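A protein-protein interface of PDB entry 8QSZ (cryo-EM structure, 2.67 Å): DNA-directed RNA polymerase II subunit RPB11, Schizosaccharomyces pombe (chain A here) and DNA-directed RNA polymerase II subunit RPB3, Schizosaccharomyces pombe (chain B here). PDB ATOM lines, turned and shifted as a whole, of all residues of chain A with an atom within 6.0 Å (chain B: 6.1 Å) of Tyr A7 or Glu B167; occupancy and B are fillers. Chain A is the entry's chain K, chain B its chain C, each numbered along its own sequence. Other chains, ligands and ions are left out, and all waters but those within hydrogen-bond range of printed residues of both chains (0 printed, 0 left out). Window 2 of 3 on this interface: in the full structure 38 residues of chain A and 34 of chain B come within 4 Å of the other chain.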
ATOM      1  N   GLU A   5      23.896  -9.225  13.785  1.00  0.00           N
ATOM      2  CA  GLU A   5      24.339  -7.839  13.737  1.00  0.00           C
ATOM      3  C   GLU A   5      24.634  -7.339  15.145  1.00  0.00           C
ATOM      4  O   GLU A   5      23.820  -7.502  16.055  1.00  0.00           O
ATOM      5  CB  GLU A   5      23.282  -6.968  13.072  1.00  0.00           C
ATOM      6  CG  GLU A   5      23.296  -7.033  11.550  1.00  0.00           C
ATOM      7  CD  GLU A   5      22.183  -7.889  10.976  1.00  0.00           C
ATOM      8  OE1 GLU A   5      22.057  -7.938   9.735  1.00  0.00           O
ATOM      9  OE2 GLU A   5      21.440  -8.520  11.758  1.00  0.00           O
ATOM     10  N   ARG A   6      25.804  -6.722  15.322  1.00  0.00           N
ATOM     11  CA  ARG A   6      26.234  -6.334  16.663  1.00  0.00           C
ATOM     12  C   ARG A   6      25.292  -5.313  17.285  1.00  0.00           C
ATOM     13  O   ARG A   6      25.204  -5.226  18.515  1.00  0.00           O
ATOM     14  CB  ARG A   6      27.658  -5.783  16.622  1.00  0.00           C
ATOM     15  CG  ARG A   6      28.723  -6.829  16.347  1.00  0.00           C
ATOM     16  CD  ARG A   6      28.990  -7.705  17.559  1.00  0.00           C
ATOM     17  NE  ARG A   6      30.028  -7.166  18.429  1.00  0.00           N
ATOM     18  CZ  ARG A   6      31.318  -7.108  18.121  1.00  0.00           C
ATOM     19  NH1 ARG A   6      31.770  -7.535  16.954  1.00  0.00           N
ATOM     20  NH2 ARG A   6      32.174  -6.611  19.005  1.00  0.00           N
ATOM     21  N   TYR A   7      24.572  -4.542  16.467  1.00  0.00           N
ATOM     22  CA  TYR A   7      23.605  -3.604  17.022  1.00  0.00           C
ATOM     23  C   TYR A   7      22.491  -4.321  17.767  1.00  0.00           C
ATOM     24  O   TYR A   7      21.766  -3.687  18.539  1.00  0.00           O
ATOM     25  CB  TYR A   7      23.020  -2.710  15.922  1.00  0.00           C
ATOM     26  CG  TYR A   7      22.213  -3.416  14.850  1.00  0.00           C
ATOM     27  CD1 TYR A   7      21.025  -4.070  15.151  1.00  0.00           C
ATOM     28  CD2 TYR A   7      22.625  -3.398  13.527  1.00  0.00           C
ATOM     29  CE1 TYR A   7      20.292  -4.701  14.177  1.00  0.00           C
ATOM     30  CE2 TYR A   7      21.890  -4.028  12.543  1.00  0.00           C
ATOM     31  CZ  TYR A   7      20.726  -4.677  12.876  1.00  0.00           C
ATOM     32  OH  TYR A   7      19.989  -5.307  11.902  1.00  0.00           O
ATOM     33  N   GLU A   8      22.335  -5.627  17.551  1.00  0.00           N
ATOM     34  CA  GLU A   8      21.355  -6.401  18.297  1.00  0.00           C
ATOM     35  C   GLU A   8      21.735  -6.547  19.760  1.00  0.00           C
ATOM     36  O   GLU A   8      20.927  -7.054  20.542  1.00  0.00           O
ATOM     37  CB  GLU A   8      21.186  -7.781  17.666  1.00  0.00           C
ATOM     38  CG  GLU A   8      20.324  -7.777  16.422  1.00  0.00           C
ATOM     39  CD  GLU A   8      20.135  -9.162  15.838  1.00  0.00           C
ATOM     40  OE1 GLU A   8      20.507 -10.148  16.510  1.00  0.00           O
ATOM     41  OE2 GLU A   8      19.612  -9.265  14.709  1.00  0.00           O
ATOM     42  N   LEU A   9      22.942  -6.140  20.142  1.00  0.00           N
ATOM     43  CA  LEU A   9      23.315  -6.083  21.547  1.00  0.00           C
ATOM     44  C   LEU A   9      22.811  -4.826  22.235  1.00  0.00           C
ATOM     45  O   LEU A   9      22.960  -4.708  23.455  1.00  0.00           O
ATOM     46  CB  LEU A   9      24.837  -6.148  21.690  1.00  0.00           C
ATOM     47  CG  LEU A   9      25.544  -7.368  21.107  1.00  0.00           C
ATOM     48  CD1 LEU A   9      27.018  -7.323  21.443  1.00  0.00           C
ATOM     49  CD2 LEU A   9      24.921  -8.645  21.630  1.00  0.00           C
ATOM     50  N   ILE A  10      22.242  -3.881  21.488  1.00  0.00           N
ATOM     51  CA  ILE A  10      21.880  -2.581  22.039  1.00  0.00           C
ATOM     52  C   ILE A  10      20.466  -2.175  21.639  1.00  0.00           C
ATOM     53  O   ILE A  10      19.890  -1.255  22.228  1.00  0.00           O
ATOM     54  CB  ILE A  10      22.909  -1.520  21.607  1.00  0.00           C
ATOM     55  CG1 ILE A  10      22.926  -1.373  20.089  1.00  0.00           C
ATOM     56  CG2 ILE A  10      24.293  -1.892  22.098  1.00  0.00           C
ATOM     57  CD1 ILE A  10      23.733  -0.205  19.610  1.00  0.00           C
ATOM     58  N   GLU A  11      19.891  -2.852  20.652  1.00  0.00           N
ATOM     59  CA  GLU A  11      18.579  -2.506  20.122  1.00  0.00           C
ATOM     60  C   GLU A  11      17.551  -3.514  20.612  1.00  0.00           C
ATOM     61  O   GLU A  11      17.801  -4.721  20.588  1.00  0.00           O
ATOM     62  CB  GLU A  11      18.594  -2.470  18.594  1.00  0.00           C
ATOM     63  CG  GLU A  11      19.426  -1.351  18.007  1.00  0.00           C
ATOM     64  CD  GLU A  11      18.800   0.009  18.212  1.00  0.00           C
ATOM     65  OE1 GLU A  11      19.522   0.935  18.632  1.00  0.00           O
ATOM     66  OE2 GLU A  11      17.589   0.155  17.958  1.00  0.00           O
ATOM     67  N   LEU A  12      16.395  -3.013  21.051  1.00  0.00           N
ATOM     68  CA  LEU A  12      15.370  -3.884  21.613  1.00  0.00           C
ATOM     69  C   LEU A  12      14.543  -4.577  20.537  1.00  0.00           C
ATOM     70  O   LEU A  12      13.967  -5.637  20.799  1.00  0.00           O
ATOM     71  CB  LEU A  12      14.451  -3.084  22.538  1.00  0.00           C
ATOM     72  CG  LEU A  12      15.084  -2.510  23.810  1.00  0.00           C
ATOM     73  CD1 LEU A  12      14.068  -1.704  24.594  1.00  0.00           C
ATOM     74  CD2 LEU A  12      15.658  -3.607  24.682  1.00  0.00           C
ATOM     75  N   MET A  13      14.464  -4.008  19.338  1.00  0.00           N
ATOM     76  CA  MET A  13      13.674  -4.592  18.254  1.00  0.00           C
ATOM     77  C   MET A  13      12.233  -4.838  18.697  1.00  0.00           C
ATOM     78  O   MET A  13      11.608  -5.837  18.336  1.00  0.00           O
ATOM     79  CB  MET A  13      14.305  -5.888  17.740  1.00  0.00           C
ATOM     80  CG  MET A  13      15.515  -5.698  16.834  1.00  0.00           C
ATOM     81  SD  MET A  13      17.008  -5.175  17.692  1.00  0.00           S
ATOM     82  CE  MET A  13      17.475  -6.699  18.507  1.00  0.00           C
ATOM     83  N   LYS A  36      18.911  -6.851  26.704  1.00  0.00           N
ATOM     84  CA  LYS A  36      20.085  -6.075  26.323  1.00  0.00           C
ATOM     85  C   LYS A  36      20.815  -5.564  27.556  1.00  0.00           C
ATOM     86  O   LYS A  36      21.278  -4.426  27.608  1.00  0.00           O
ATOM     87  CB  LYS A  36      19.706  -4.923  25.394  1.00  0.00           C
ATOM     88  CG  LYS A  36      18.760  -5.314  24.279  1.00  0.00           C
ATOM     89  CD  LYS A  36      19.357  -6.351  23.347  1.00  0.00           C
ATOM     90  CE  LYS A  36      18.271  -7.082  22.584  1.00  0.00           C
ATOM     91  NZ  LYS A  36      18.793  -7.778  21.384  1.00  0.00           N
ATOM     92  N   ALA B  38      33.241  -1.252  27.996  1.00  0.00           N
ATOM     93  CA  ALA B  38      32.220  -1.760  27.085  1.00  0.00           C
ATOM     94  C   ALA B  38      31.194  -0.748  26.580  1.00  0.00           C
ATOM     95  O   ALA B  38      30.635  -0.947  25.498  1.00  0.00           O
ATOM     96  CB  ALA B  38      31.470  -2.905  27.764  1.00  0.00           C
ATOM     97  N   ARG B  88      21.032   6.302  13.930  1.00  0.00           N
ATOM     98  CA  ARG B  88      19.775   5.565  13.933  1.00  0.00           C
ATOM     99  C   ARG B  88      18.668   6.358  14.614  1.00  0.00           C
ATOM    100  O   ARG B  88      17.508   6.294  14.190  1.00  0.00           O
ATOM    101  CB  ARG B  88      19.969   4.214  14.620  1.00  0.00           C
ATOM    102  CG  ARG B  88      20.601   4.309  16.000  1.00  0.00           C
ATOM    103  CD  ARG B  88      20.791   2.944  16.616  1.00  0.00           C
ATOM    104  NE  ARG B  88      22.039   2.857  17.367  1.00  0.00           N
ATOM    105  CZ  ARG B  88      22.149   3.013  18.680  1.00  0.00           C
ATOM    106  NH1 ARG B  88      21.098   3.270  19.441  1.00  0.00           N
ATOM    107  NH2 ARG B  88      23.349   2.913  19.244  1.00  0.00           N
ATOM    108  N   LYS B 162      28.668   7.639  16.228  1.00  0.00           N
ATOM    109  CA  LYS B 162      28.744   7.407  17.660  1.00  0.00           C
ATOM    110  C   LYS B 162      28.466   5.937  17.955  1.00  0.00           C
ATOM    111  O   LYS B 162      27.657   5.293  17.283  1.00  0.00           O
ATOM    112  CB  LYS B 162      27.733   8.303  18.379  1.00  0.00           C
ATOM    113  CG  LYS B 162      27.847   8.350  19.880  1.00  0.00           C
ATOM    114  CD  LYS B 162      26.812   9.297  20.442  1.00  0.00           C
ATOM    115  CE  LYS B 162      26.879   9.375  21.948  1.00  0.00           C
ATOM    116  NZ  LYS B 162      25.793  10.220  22.499  1.00  0.00           N
ATOM    117  N   GLY B 163      29.151   5.404  18.957  1.00  0.00           N
ATOM    118  CA  GLY B 163      28.975   4.003  19.288  1.00  0.00           C
ATOM    119  C   GLY B 163      29.756   3.641  20.527  1.00  0.00           C
ATOM    120  O   GLY B 163      30.420   4.479  21.140  1.00  0.00           O
ATOM    121  N   ILE B 164      29.661   2.362  20.888  1.00  0.00           N
ATOM    122  CA  ILE B 164      30.271   1.816  22.091  1.00  0.00           C
ATOM    123  C   ILE B 164      31.023   0.545  21.715  1.00  0.00           C
ATOM    124  O   ILE B 164      30.819  -0.030  20.648  1.00  0.00           O
ATOM    125  CB  ILE B 164      29.229   1.528  23.192  1.00  0.00           C
ATOM    126  CG1 ILE B 164      28.109   0.642  22.649  1.00  0.00           C
ATOM    127  CG2 ILE B 164      28.648   2.820  23.713  1.00  0.00           C
ATOM    128  CD1 ILE B 164      27.237   0.048  23.711  1.00  0.00           C
ATOM    129  N   ALA B 165      31.905   0.108  22.615  1.00  0.00           N
ATOM    130  CA  ALA B 165      32.754  -1.045  22.340  1.00  0.00           C
ATOM    131  C   ALA B 165      31.980  -2.351  22.242  1.00  0.00           C
ATOM    132  O   ALA B 165      32.550  -3.353  21.802  1.00  0.00           O
ATOM    133  CB  ALA B 165      33.828  -1.172  23.414  1.00  0.00           C
ATOM    134  N   LYS B 166      30.715  -2.381  22.652  1.00  0.00           N
ATOM    135  CA  LYS B 166      29.930  -3.597  22.488  1.00  0.00           C
ATOM    136  C   LYS B 166      29.643  -3.868  21.019  1.00  0.00           C
ATOM    137  O   LYS B 166      29.633  -5.025  20.586  1.00  0.00           O
ATOM    138  CB  LYS B 166      28.629  -3.494  23.278  1.00  0.00           C
ATOM    139  CG  LYS B 166      28.816  -3.635  24.776  1.00  0.00           C
ATOM    140  CD  LYS B 166      27.644  -4.333  25.440  1.00  0.00           C
ATOM    141  CE  LYS B 166      26.662  -3.327  25.985  1.00  0.00           C
ATOM    142  NZ  LYS B 166      25.414  -3.953  26.475  1.00  0.00           N
ATOM    143  N   GLU B 167      29.392  -2.816  20.241  1.00  0.00           N
ATOM    144  CA  GLU B 167      29.130  -2.993  18.820  1.00  0.00           C
ATOM    145  C   GLU B 167      30.406  -3.235  18.029  1.00  0.00           C
ATOM    146  O   GLU B 167      30.381  -3.956  17.028  1.00  0.00           O
ATOM    147  CB  GLU B 167      28.394  -1.777  18.270  1.00  0.00           C
ATOM    148  CG  GLU B 167      27.837  -1.988  16.880  1.00  0.00           C
ATOM    149  CD  GLU B 167      26.895  -0.890  16.461  1.00  0.00           C
ATOM    150  OE1 GLU B 167      26.666   0.034  17.266  1.00  0.00           O
ATOM    151  OE2 GLU B 167      26.381  -0.951  15.326  1.00  0.00           O
ATOM    152  N   HIS B 168      31.516  -2.635  18.445  1.00  0.00           N
ATOM    153  CA  HIS B 168      32.804  -2.872  17.810  1.00  0.00           C
ATOM    154  C   HIS B 168      33.885  -2.247  18.667  1.00  0.00           C
ATOM    155  O   HIS B 168      33.738  -1.115  19.122  1.00  0.00           O
ATOM    156  CB  HIS B 168      32.856  -2.290  16.393  1.00  0.00           C
ATOM    157  CG  HIS B 168      33.987  -2.820  15.570  1.00  0.00           C
ATOM    158  ND1 HIS B 168      35.208  -2.191  15.491  1.00  0.00           N
ATOM    159  CD2 HIS B 168      34.085  -3.926  14.799  1.00  0.00           C
ATOM    160  CE1 HIS B 168      36.009  -2.882  14.703  1.00  0.00           C
ATOM    161  NE2 HIS B 168      35.350  -3.937  14.267  1.00  0.00           N
ATOM    162  N   ALA B 169      34.978  -2.979  18.856  1.00  0.00           N
ATOM    163  CA  ALA B 169      36.065  -2.544  19.722  1.00  0.00           C
ATOM    164  C   ALA B 169      36.710  -1.246  19.268  1.00  0.00           C
ATOM    165  O   ALA B 169      37.573  -0.729  19.984  1.00  0.00           O
ATOM    166  CB  ALA B 169      37.125  -3.639  19.804  1.00  0.00           C
ATOM    167  N   TRP B 171      35.153   1.564  19.025  1.00  0.00           N
ATOM    168  CA  TRP B 171      34.509   2.606  19.807  1.00  0.00           C
ATOM    169  C   TRP B 171      34.933   2.589  21.268  1.00  0.00           C
ATOM    170  O   TRP B 171      34.301   3.256  22.093  1.00  0.00           O
ATOM    171  CB  TRP B 171      32.995   2.465  19.703  1.00  0.00           C
ATOM    172  CG  TRP B 171      32.427   3.053  18.464  1.00  0.00           C
ATOM    173  CD1 TRP B 171      32.496   4.350  18.076  1.00  0.00           C
ATOM    174  CD2 TRP B 171      31.689   2.369  17.448  1.00  0.00           C
ATOM    175  NE1 TRP B 171      31.852   4.522  16.881  1.00  0.00           N
ATOM    176  CE2 TRP B 171      31.347   3.318  16.474  1.00  0.00           C
ATOM    177  CE3 TRP B 171      31.289   1.044  17.269  1.00  0.00           C
ATOM    178  CZ2 TRP B 171      30.624   2.990  15.341  1.00  0.00           C
ATOM    179  CZ3 TRP B 171      30.573   0.721  16.142  1.00  0.00           C
ATOM    180  CH2 TRP B 171      30.245   1.689  15.193  1.00  0.00           C
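NE of Arg A6 lies within hydrogen-bond range of O of Lys B166.
NH1 of Arg B88 lies within salt-bridge range of OE1 of Glu A11 (2.9 Å).
The backbone carbonyl oxygen (O) of Glu A11 sits close to the side-chain amino group (NZ) of Lys A36 (3.3 Å).
The backbone carbonyl oxygen of Ala B38 lies within hydrogen-bond range of the backbone NH of Lys B166, at 3.2 Å.
Among the printed residues, pairs that only touch across the chains: Ile A10 with Arg B88, Arg A6 with Glu B167, Leu A9 with Lys B166, Ile A10 with Glu B167, Tyr A7 with Glu B167, Ile A10 with Ile B164 and Arg A6 with His B168.
Glu A5 touches none of the printed residues of chain B.
Of the printed residues of chain B, Arg A6 touches Lys B166 (3.1 Å), Glu B167 (3.3 Å) and His B168 (3.98 Å).
Tyr A7 touches just one residue of chain B: Glu B167.
Of the printed residues of chain B, Ile A10 touches Arg B88, Ile B164 and Glu B167.
Of the printed residues of chain B, Glu A11 touches Arg B88.
Leu A12 touches none of the printed residues of chain B.
The nearest residue of chain A that does not touch Glu B167 is Leu A9 (5.2 Å).
Of the 10 printed residues of chain A, 5 touch a printed residue of chain B.
Printed residues of chain A that touch a printed residue of chain B: Arg A6, Tyr A7, Leu A9, Ile A10 and Glu A11.
Printed residues of chain B that touch a printed residue of chain A: Arg B88, Ile B164, Lys B166, Glu B167 and His B168.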
